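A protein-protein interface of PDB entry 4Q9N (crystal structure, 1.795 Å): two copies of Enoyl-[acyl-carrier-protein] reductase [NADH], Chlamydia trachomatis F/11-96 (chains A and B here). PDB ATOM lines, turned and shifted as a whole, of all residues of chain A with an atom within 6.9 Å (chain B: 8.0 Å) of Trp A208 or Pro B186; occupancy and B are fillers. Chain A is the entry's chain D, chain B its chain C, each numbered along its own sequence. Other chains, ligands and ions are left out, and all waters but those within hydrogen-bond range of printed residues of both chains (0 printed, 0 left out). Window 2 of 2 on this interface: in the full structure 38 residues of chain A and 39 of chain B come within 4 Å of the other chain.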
ATOM      1  N   ASP A 202      -5.743 -14.494  33.927  1.00  0.00           N
ATOM      2  CA  ASP A 202      -5.168 -15.017  32.685  1.00  0.00           C
ATOM      3  C   ASP A 202      -6.233 -15.120  31.592  1.00  0.00           C
ATOM      4  O   ASP A 202      -5.937 -14.882  30.418  1.00  0.00           O
ATOM      5  CB  ASP A 202      -4.500 -16.365  32.919  1.00  0.00           C
ATOM      6  CG  ASP A 202      -3.275 -16.266  33.817  1.00  0.00           C
ATOM      7  OD1 ASP A 202      -2.756 -15.142  34.013  1.00  0.00           O
ATOM      8  OD2 ASP A 202      -2.820 -17.323  34.335  1.00  0.00           O
ATOM      9  N   THR A 203      -7.469 -15.462  31.966  1.00  0.00           N
ATOM     10  CA  THR A 203      -8.553 -15.534  30.972  1.00  0.00           C
ATOM     11  C   THR A 203      -8.712 -14.226  30.189  1.00  0.00           C
ATOM     12  O   THR A 203      -8.874 -14.241  28.965  1.00  0.00           O
ATOM     13  CB  THR A 203      -9.908 -15.890  31.601  1.00  0.00           C
ATOM     14  OG1 THR A 203      -9.863 -17.226  32.103  1.00  0.00           O
ATOM     15  CG2 THR A 203     -11.044 -15.786  30.545  1.00  0.00           C
ATOM     16  N   LYS A 204      -8.667 -13.100  30.896  1.00  0.00           N
ATOM     17  CA  LYS A 204      -8.812 -11.784  30.257  1.00  0.00           C
ATOM     18  C   LYS A 204      -7.602 -11.418  29.374  1.00  0.00           C
ATOM     19  O   LYS A 204      -7.754 -10.930  28.243  1.00  0.00           O
ATOM     20  CB  LYS A 204      -9.028 -10.710  31.316  1.00  0.00           C
ATOM     21  CG  LYS A 204     -10.286 -10.921  32.133  1.00  0.00           C
ATOM     22  CD  LYS A 204     -10.328  -9.977  33.303  1.00  0.00           C
ATOM     23  CE  LYS A 204     -11.531 -10.291  34.170  1.00  0.00           C
ATOM     24  NZ  LYS A 204     -11.570 -11.747  34.492  1.00  0.00           N
ATOM     25  N   VAL A 205      -6.404 -11.661  29.902  1.00  0.00           N
ATOM     26  CA  VAL A 205      -5.171 -11.332  29.195  1.00  0.00           C
ATOM     27  C   VAL A 205      -5.037 -12.209  27.951  1.00  0.00           C
ATOM     28  O   VAL A 205      -4.751 -11.719  26.849  1.00  0.00           O
ATOM     29  CB  VAL A 205      -3.926 -11.508  30.132  1.00  0.00           C
ATOM     30  CG1 VAL A 205      -2.644 -11.445  29.335  1.00  0.00           C
ATOM     31  CG2 VAL A 205      -3.938 -10.407  31.204  1.00  0.00           C
ATOM     32  N   LEU A 206      -5.290 -13.500  28.119  1.00  0.00           N
ATOM     33  CA  LEU A 206      -5.190 -14.421  26.992  1.00  0.00           C
ATOM     34  C   LEU A 206      -6.287 -14.185  25.943  1.00  0.00           C
ATOM     35  O   LEU A 206      -6.065 -14.439  24.764  1.00  0.00           O
ATOM     36  CB  LEU A 206      -5.198 -15.871  27.464  1.00  0.00           C
ATOM     37  CG  LEU A 206      -4.006 -16.253  28.350  1.00  0.00           C
ATOM     38  CD1 LEU A 206      -4.236 -17.632  28.934  1.00  0.00           C
ATOM     39  CD2 LEU A 206      -2.715 -16.210  27.539  1.00  0.00           C
ATOM     40  N   ALA A 207      -7.454 -13.700  26.364  1.00  0.00           N
ATOM     41  CA  ALA A 207      -8.507 -13.342  25.396  1.00  0.00           C
ATOM     42  C   ALA A 207      -7.990 -12.286  24.430  1.00  0.00           C
ATOM     43  O   ALA A 207      -8.232 -12.370  23.229  1.00  0.00           O
ATOM     44  CB  ALA A 207      -9.774 -12.848  26.095  1.00  0.00           C
ATOM     45  N   TRP A 208      -7.264 -11.305  24.953  1.00  0.00           N
ATOM     46  CA  TRP A 208      -6.644 -10.315  24.083  1.00  0.00           C
ATOM     47  C   TRP A 208      -5.501 -10.917  23.273  1.00  0.00           C
ATOM     48  O   TRP A 208      -5.419 -10.718  22.072  1.00  0.00           O
ATOM     49  CB  TRP A 208      -6.120  -9.113  24.864  1.00  0.00           C
ATOM     50  CG  TRP A 208      -5.814  -7.945  23.949  1.00  0.00           C
ATOM     51  CD1 TRP A 208      -6.719  -7.074  23.391  1.00  0.00           C
ATOM     52  CD2 TRP A 208      -4.530  -7.553  23.458  1.00  0.00           C
ATOM     53  NE1 TRP A 208      -6.068  -6.154  22.604  1.00  0.00           N
ATOM     54  CE2 TRP A 208      -4.724  -6.426  22.629  1.00  0.00           C
ATOM     55  CE3 TRP A 208      -3.233  -8.038  23.645  1.00  0.00           C
ATOM     56  CZ2 TRP A 208      -3.671  -5.782  21.991  1.00  0.00           C
ATOM     57  CZ3 TRP A 208      -2.189  -7.396  23.012  1.00  0.00           C
ATOM     58  CH2 TRP A 208      -2.412  -6.280  22.195  1.00  0.00           C
ATOM     59  N   GLU A 209      -4.600 -11.637  23.941  1.00  0.00           N
ATOM     60  CA  GLU A 209      -3.403 -12.100  23.264  1.00  0.00           C
ATOM     61  C   GLU A 209      -3.721 -13.166  22.219  1.00  0.00           C
ATOM     62  O   GLU A 209      -3.181 -13.134  21.121  1.00  0.00           O
ATOM     63  CB  GLU A 209      -2.374 -12.604  24.278  1.00  0.00           C
ATOM     64  CG  GLU A 209      -1.747 -11.500  25.122  1.00  0.00           C
ATOM     65  CD  GLU A 209      -0.707 -12.042  26.100  1.00  0.00           C
ATOM     66  OE1 GLU A 209      -0.576 -13.273  26.180  1.00  0.00           O
ATOM     67  OE2 GLU A 209      -0.038 -11.248  26.796  1.00  0.00           O
ATOM     68  N   ALA A 210      -4.601 -14.098  22.559  1.00  0.00           N
ATOM     69  CA  ALA A 210      -4.937 -15.190  21.656  1.00  0.00           C
ATOM     70  C   ALA A 210      -5.929 -14.696  20.603  1.00  0.00           C
ATOM     71  O   ALA A 210      -5.929 -15.166  19.455  1.00  0.00           O
ATOM     72  CB  ALA A 210      -5.526 -16.352  22.424  1.00  0.00           C
ATOM     73  N   GLY A 211      -6.781 -13.757  21.002  1.00  0.00           N
ATOM     74  CA  GLY A 211      -7.701 -13.135  20.062  1.00  0.00           C
ATOM     75  C   GLY A 211      -6.934 -12.434  18.959  1.00  0.00           C
ATOM     76  O   GLY A 211      -7.194 -12.642  17.772  1.00  0.00           O
ATOM     77  N   ARG A 212      -5.963 -11.616  19.334  1.00  0.00           N
ATOM     78  CA  ARG A 212      -5.202 -10.896  18.319  1.00  0.00           C
ATOM     79  C   ARG A 212      -4.240 -11.792  17.538  1.00  0.00           C
ATOM     80  O   ARG A 212      -4.010 -11.567  16.351  1.00  0.00           O
ATOM     81  CB  ARG A 212      -4.453  -9.718  18.928  1.00  0.00           C
ATOM     82  CG  ARG A 212      -5.363  -8.689  19.572  1.00  0.00           C
ATOM     83  CD  ARG A 212      -6.388  -8.125  18.588  1.00  0.00           C
ATOM     84  NE  ARG A 212      -7.162  -7.051  19.209  1.00  0.00           N
ATOM     85  CZ  ARG A 212      -6.823  -5.766  19.162  1.00  0.00           C
ATOM     86  NH1 ARG A 212      -5.732  -5.389  18.507  1.00  0.00           N
ATOM     87  NH2 ARG A 212      -7.576  -4.856  19.769  1.00  0.00           N
ATOM     88  N   ARG A 213      -3.673 -12.801  18.192  1.00  0.00           N
ATOM     89  CA  ARG A 213      -2.690 -13.647  17.510  1.00  0.00           C
ATOM     90  C   ARG A 213      -3.298 -14.693  16.568  1.00  0.00           C
ATOM     91  O   ARG A 213      -2.780 -14.916  15.457  1.00  0.00           O
ATOM     92  CB  ARG A 213      -1.741 -14.320  18.524  1.00  0.00           C
ATOM     93  CG  ARG A 213      -0.624 -15.104  17.857  1.00  0.00           C
ATOM     94  CD  ARG A 213       0.403 -15.692  18.847  1.00  0.00           C
ATOM     95  NE  ARG A 213       1.023 -14.694  19.728  1.00  0.00           N
ATOM     96  CZ  ARG A 213       1.977 -14.979  20.617  1.00  0.00           C
ATOM     97  NH1 ARG A 213       2.422 -16.227  20.746  1.00  0.00           N
ATOM     98  NH2 ARG A 213       2.492 -14.019  21.382  1.00  0.00           N
ATOM     99  N   VAL A 216      -8.637 -16.560  18.364  1.00  0.00           N
ATOM    100  CA  VAL A 216      -9.226 -17.546  19.261  1.00  0.00           C
ATOM    101  C   VAL A 216      -9.957 -16.839  20.403  1.00  0.00           C
ATOM    102  O   VAL A 216      -9.489 -15.811  20.892  1.00  0.00           O
ATOM    103  CB  VAL A 216      -8.107 -18.471  19.847  1.00  0.00           C
ATOM    104  CG1 VAL A 216      -8.605 -19.312  21.011  1.00  0.00           C
ATOM    105  CG2 VAL A 216      -7.509 -19.373  18.744  1.00  0.00           C
ATOM    106  N   VAL A 218     -11.520 -16.956  24.405  1.00  0.00           N
ATOM    107  CA  VAL A 218     -11.046 -17.572  25.639  1.00  0.00           C
ATOM    108  C   VAL A 218     -12.030 -17.226  26.753  1.00  0.00           C
ATOM    109  O   VAL A 218     -12.118 -16.071  27.154  1.00  0.00           O
ATOM    110  CB  VAL A 218      -9.632 -17.046  26.042  1.00  0.00           C
ATOM    111  CG1 VAL A 218      -9.208 -17.647  27.371  1.00  0.00           C
ATOM    112  CG2 VAL A 218      -8.573 -17.358  24.975  1.00  0.00           C
ATOM    113  N   THR A 275     -15.975 -13.144  24.511  1.00  0.00           N
ATOM    114  CA  THR A 275     -14.606 -13.533  24.848  1.00  0.00           C
ATOM    115  C   THR A 275     -14.096 -12.840  26.113  1.00  0.00           C
ATOM    116  O   THR A 275     -14.492 -11.722  26.427  1.00  0.00           O
ATOM    117  CB  THR A 275     -13.628 -13.356  23.628  1.00  0.00           C
ATOM    118  OG1 THR A 275     -12.409 -14.060  23.870  1.00  0.00           O
ATOM    119  CG2 THR A 275     -13.316 -11.879  23.349  1.00  0.00           C
ATOM    120  N   GLY A 276     -13.228 -13.525  26.861  1.00  0.00           N
ATOM    121  CA  GLY A 276     -12.719 -12.966  28.095  1.00  0.00           C
ATOM    122  C   GLY A 276     -13.730 -13.031  29.222  1.00  0.00           C
ATOM    123  O   GLY A 276     -13.529 -12.442  30.280  1.00  0.00           O
ATOM    124  N   ILE B 133       8.836 -10.056  32.188  1.00  0.00           N
ATOM    125  CA  ILE B 133       7.776  -9.052  32.031  1.00  0.00           C
ATOM    126  C   ILE B 133       7.642  -8.518  30.601  1.00  0.00           C
ATOM    127  O   ILE B 133       6.586  -8.003  30.219  1.00  0.00           O
ATOM    128  CB  ILE B 133       7.952  -7.870  33.025  1.00  0.00           C
ATOM    129  CG1 ILE B 133       6.610  -7.152  33.243  1.00  0.00           C
ATOM    130  CG2 ILE B 133       9.064  -6.926  32.558  1.00  0.00           C
ATOM    131  CD1 ILE B 133       6.695  -5.977  34.190  1.00  0.00           C
ATOM    132  N   LYS B 135       7.638 -10.305  28.006  1.00  0.00           N
ATOM    133  CA  LYS B 135       7.005 -11.342  27.205  1.00  0.00           C
ATOM    134  C   LYS B 135       5.491 -11.306  27.353  1.00  0.00           C
ATOM    135  O   LYS B 135       4.977 -11.116  28.463  1.00  0.00           O
ATOM    136  CB  LYS B 135       7.517 -12.724  27.639  1.00  0.00           C
ATOM    137  CG  LYS B 135       8.815 -13.171  26.965  1.00  0.00           C
ATOM    138  CD  LYS B 135       9.879 -12.106  27.094  1.00  0.00           C
ATOM    139  CE  LYS B 135      10.996 -12.270  26.088  1.00  0.00           C
ATOM    140  NZ  LYS B 135      12.068 -11.240  26.285  1.00  0.00           N
ATOM    141  N   PRO B 136       4.766 -11.484  26.235  1.00  0.00           N
ATOM    142  CA  PRO B 136       3.339 -11.803  26.307  1.00  0.00           C
ATOM    143  C   PRO B 136       3.125 -12.999  27.231  1.00  0.00           C
ATOM    144  O   PRO B 136       3.993 -13.864  27.320  1.00  0.00           O
ATOM    145  CB  PRO B 136       3.005 -12.202  24.866  1.00  0.00           C
ATOM    146  CG  PRO B 136       3.997 -11.462  24.030  1.00  0.00           C
ATOM    147  CD  PRO B 136       5.258 -11.458  24.844  1.00  0.00           C
ATOM    148  N   LEU B 138       1.211 -15.452  26.815  1.00  0.00           N
ATOM    149  CA  LEU B 138       1.230 -16.613  25.926  1.00  0.00           C
ATOM    150  C   LEU B 138       2.624 -17.193  25.721  1.00  0.00           C
ATOM    151  O   LEU B 138       2.766 -18.386  25.458  1.00  0.00           O
ATOM    152  CB  LEU B 138       0.691 -16.239  24.541  1.00  0.00           C
ATOM    153  CG  LEU B 138      -0.749 -16.587  24.190  1.00  0.00           C
ATOM    154  CD1 LEU B 138      -1.013 -16.159  22.756  1.00  0.00           C
ATOM    155  CD2 LEU B 138      -1.012 -18.066  24.379  1.00  0.00           C
ATOM    156  N   ALA B 180      -3.888  -4.082  36.450  1.00  0.00           N
ATOM    157  CA  ALA B 180      -3.726  -5.177  35.490  1.00  0.00           C
ATOM    158  C   ALA B 180      -3.998  -6.552  36.110  1.00  0.00           C
ATOM    159  O   ALA B 180      -4.035  -7.564  35.415  1.00  0.00           O
ATOM    160  CB  ALA B 180      -2.342  -5.140  34.880  1.00  0.00           C
ATOM    161  N   ARG B 183      -7.914  -6.661  35.029  1.00  0.00           N
ATOM    162  CA  ARG B 183      -8.286  -6.145  33.708  1.00  0.00           C
ATOM    163  C   ARG B 183      -7.077  -6.307  32.805  1.00  0.00           C
ATOM    164  O   ARG B 183      -5.940  -6.196  33.270  1.00  0.00           O
ATOM    165  CB  ARG B 183      -8.688  -4.682  33.781  1.00  0.00           C
ATOM    166  CG  ARG B 183      -9.927  -4.400  34.611  1.00  0.00           C
ATOM    167  CD  ARG B 183     -10.232  -2.913  34.595  1.00  0.00           C
ATOM    168  NE  ARG B 183     -10.904  -2.480  35.816  1.00  0.00           N
ATOM    169  CZ  ARG B 183     -11.049  -1.208  36.174  1.00  0.00           C
ATOM    170  NH1 ARG B 183     -10.568  -0.245  35.400  1.00  0.00           N
ATOM    171  NH2 ARG B 183     -11.673  -0.903  37.307  1.00  0.00           N
ATOM    172  N   ALA B 184      -7.304  -6.600  31.525  1.00  0.00           N
ATOM    173  CA  ALA B 184      -6.203  -6.946  30.635  1.00  0.00           C
ATOM    174  C   ALA B 184      -5.395  -5.733  30.194  1.00  0.00           C
ATOM    175  O   ALA B 184      -5.917  -4.835  29.530  1.00  0.00           O
ATOM    176  CB  ALA B 184      -6.709  -7.724  29.423  1.00  0.00           C
ATOM    177  N   VAL B 185      -4.115  -5.717  30.564  1.00  0.00           N
ATOM    178  CA  VAL B 185      -3.207  -4.651  30.144  1.00  0.00           C
ATOM    179  C   VAL B 185      -2.032  -5.246  29.371  1.00  0.00           C
ATOM    180  O   VAL B 185      -1.096  -5.778  29.966  1.00  0.00           O
ATOM    181  CB  VAL B 185      -2.665  -3.827  31.338  1.00  0.00           C
ATOM    182  CG1 VAL B 185      -1.663  -2.775  30.852  1.00  0.00           C
ATOM    183  CG2 VAL B 185      -3.820  -3.159  32.098  1.00  0.00           C
ATOM    184  N   PRO B 186      -2.102  -5.188  28.040  1.00  0.00           N
ATOM    185  CA  PRO B 186      -1.003  -5.640  27.182  1.00  0.00           C
ATOM    186  C   PRO B 186       0.305  -4.966  27.592  1.00  0.00           C
ATOM    187  O   PRO B 186       0.327  -3.749  27.756  1.00  0.00           O
ATOM    188  CB  PRO B 186      -1.434  -5.161  25.797  1.00  0.00           C
ATOM    189  CG  PRO B 186      -2.933  -5.174  25.861  1.00  0.00           C
ATOM    190  CD  PRO B 186      -3.271  -4.738  27.258  1.00  0.00           C
ATOM    191  N   GLY B 187       1.363  -5.747  27.791  1.00  0.00           N
ATOM    192  CA  GLY B 187       2.636  -5.185  28.212  1.00  0.00           C
ATOM    193  C   GLY B 187       2.989  -5.530  29.645  1.00  0.00           C
ATOM    194  O   GLY B 187       4.156  -5.475  30.034  1.00  0.00           O
ATOM    195  N   TYR B 188       1.984  -5.883  30.439  1.00  0.00           N
ATOM    196  CA  TYR B 188       2.227  -6.328  31.809  1.00  0.00           C
ATOM    197  C   TYR B 188       2.413  -7.840  31.767  1.00  0.00           C
ATOM    198  O   TYR B 188       1.534  -8.601  32.167  1.00  0.00           O
ATOM    199  CB  TYR B 188       1.046  -5.946  32.708  1.00  0.00           C
ATOM    200  CG  TYR B 188       1.374  -5.816  34.186  1.00  0.00           C
ATOM    201  CD1 TYR B 188       2.346  -4.923  34.626  1.00  0.00           C
ATOM    202  CD2 TYR B 188       0.685  -6.559  35.141  1.00  0.00           C
ATOM    203  CE1 TYR B 188       2.637  -4.785  35.978  1.00  0.00           C
ATOM    204  CE2 TYR B 188       0.963  -6.424  36.494  1.00  0.00           C
ATOM    205  CZ  TYR B 188       1.949  -5.542  36.906  1.00  0.00           C
ATOM    206  OH  TYR B 188       2.244  -5.412  38.252  1.00  0.00           O
ATOM    207  N   GLY B 189       3.562  -8.273  31.249  1.00  0.00           N
ATOM    208  CA  GLY B 189       3.745  -9.669  30.902  1.00  0.00           C
ATOM    209  C   GLY B 189       4.453 -10.478  31.967  1.00  0.00           C
ATOM    210  O   GLY B 189       4.569 -10.049  33.115  1.00  0.00           O
ATOM    211  N   PHE B 236       8.784   2.041  29.058  1.00  0.00           N
ATOM    212  CA  PHE B 236       7.802   3.006  28.565  1.00  0.00           C
ATOM    213  C   PHE B 236       6.967   3.621  29.691  1.00  0.00           C
ATOM    214  O   PHE B 236       5.819   4.005  29.478  1.00  0.00           O
ATOM    215  CB  PHE B 236       6.884   2.348  27.533  1.00  0.00           C
ATOM    216  CG  PHE B 236       6.278   1.051  27.997  1.00  0.00           C
ATOM    217  CD1 PHE B 236       6.929  -0.156  27.771  1.00  0.00           C
ATOM    218  CD2 PHE B 236       5.056   1.033  28.653  1.00  0.00           C
ATOM    219  CE1 PHE B 236       6.373  -1.355  28.198  1.00  0.00           C
ATOM    220  CE2 PHE B 236       4.495  -0.159  29.081  1.00  0.00           C
ATOM    221  CZ  PHE B 236       5.155  -1.354  28.856  1.00  0.00           C
ATOM    222  N   ARG B 239       5.389   7.114  29.027  1.00  0.00           N
ATOM    223  CA  ARG B 239       4.178   7.145  28.207  1.00  0.00           C
ATOM    224  C   ARG B 239       2.961   6.748  29.025  1.00  0.00           C
ATOM    225  O   ARG B 239       1.853   7.187  28.747  1.00  0.00           O
ATOM    226  CB  ARG B 239       4.291   6.211  26.998  1.00  0.00           C
ATOM    227  CG  ARG B 239       5.223   6.689  25.900  1.00  0.00           C
ATOM    228  CD  ARG B 239       5.068   5.823  24.650  1.00  0.00           C
ATOM    229  NE  ARG B 239       4.941   4.406  24.991  1.00  0.00           N
ATOM    230  CZ  ARG B 239       4.038   3.582  24.464  1.00  0.00           C
ATOM    231  NH1 ARG B 239       3.176   4.028  23.555  1.00  0.00           N
ATOM    232  NH2 ARG B 239       4.000   2.311  24.842  1.00  0.00           N
ATOM    233  N   MET B 240       3.162   5.890  30.020  1.00  0.00           N
ATOM    234  CA  MET B 240       2.067   5.483  30.882  1.00  0.00           C
ATOM    235  C   MET B 240       1.683   6.623  31.807  1.00  0.00           C
ATOM    236  O   MET B 240       0.510   6.821  32.115  1.00  0.00           O
ATOM    237  CB  MET B 240       2.447   4.256  31.718  1.00  0.00           C
ATOM    238  CG  MET B 240       2.486   2.939  30.953  1.00  0.00           C
ATOM    239  SD  MET B 240       0.887   2.363  30.325  1.00  0.00           S
ATOM    240  CE  MET B 240      -0.239   3.041  31.524  1.00  0.00           C
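Trp A208 touches just one residue of chain B: Pro B186. No residue of chain B comes within 4 Å of Ala A207. Of the printed residues of chain B, Lys A204 touches Ala B184. Printed residues of chain B within 4 Å of Val A205: Ala B184. Of the printed residues of chain B, Leu A206 touches Leu B138 (3.9 Å). Of the printed residues of chain A, Ala B184 touches Lys A204 and Val A205. Lys B135 touches none of the printed residues of chain A. Ala B180 touches none of the printed residues of chain A.
The backbone NH (N) of Leu B138 is in hydrogen-bond range of the side-chain carboxylate (OE1) of Glu A209, 2.9 Å away.
Lys A204 touches Ala B184. Ala B184 touches Val A205 (CB to CA, 3.9 Å). Leu A206 touches Leu B138 (CD2 to CG, 3.9 Å). Trp A208 touches Pro B186. Pro B136 touches Glu A209 (CA to OE2, 3.5 Å). Arg A213 touches Pro B136. CZ of Arg A213 touches CD1 of Leu B138 (3.9 Å).
Printed residues of chain A that touch a printed residue of chain B: Lys A204, Val A205, Leu A206, Trp A208, Glu A209 and Arg A213. Hydrophobic or aromatic side chains of chain A that line the printed part of chain B: Leu A206 and Trp A208. Hydrophobic or aromatic side chains of chain B that line the printed part of chain A: Pro B136, Leu B138, Ala B184 and Pro B186. Among the printed residues, no Asp or Glu carboxylate lies within 4 Å of a Lys or Arg side-chain nitrogen of the other chain.
No position is printed for both chains. Of the 8 pairs that touch across the chains among the printed residues, none has its exchanged pair printed and touching as well.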
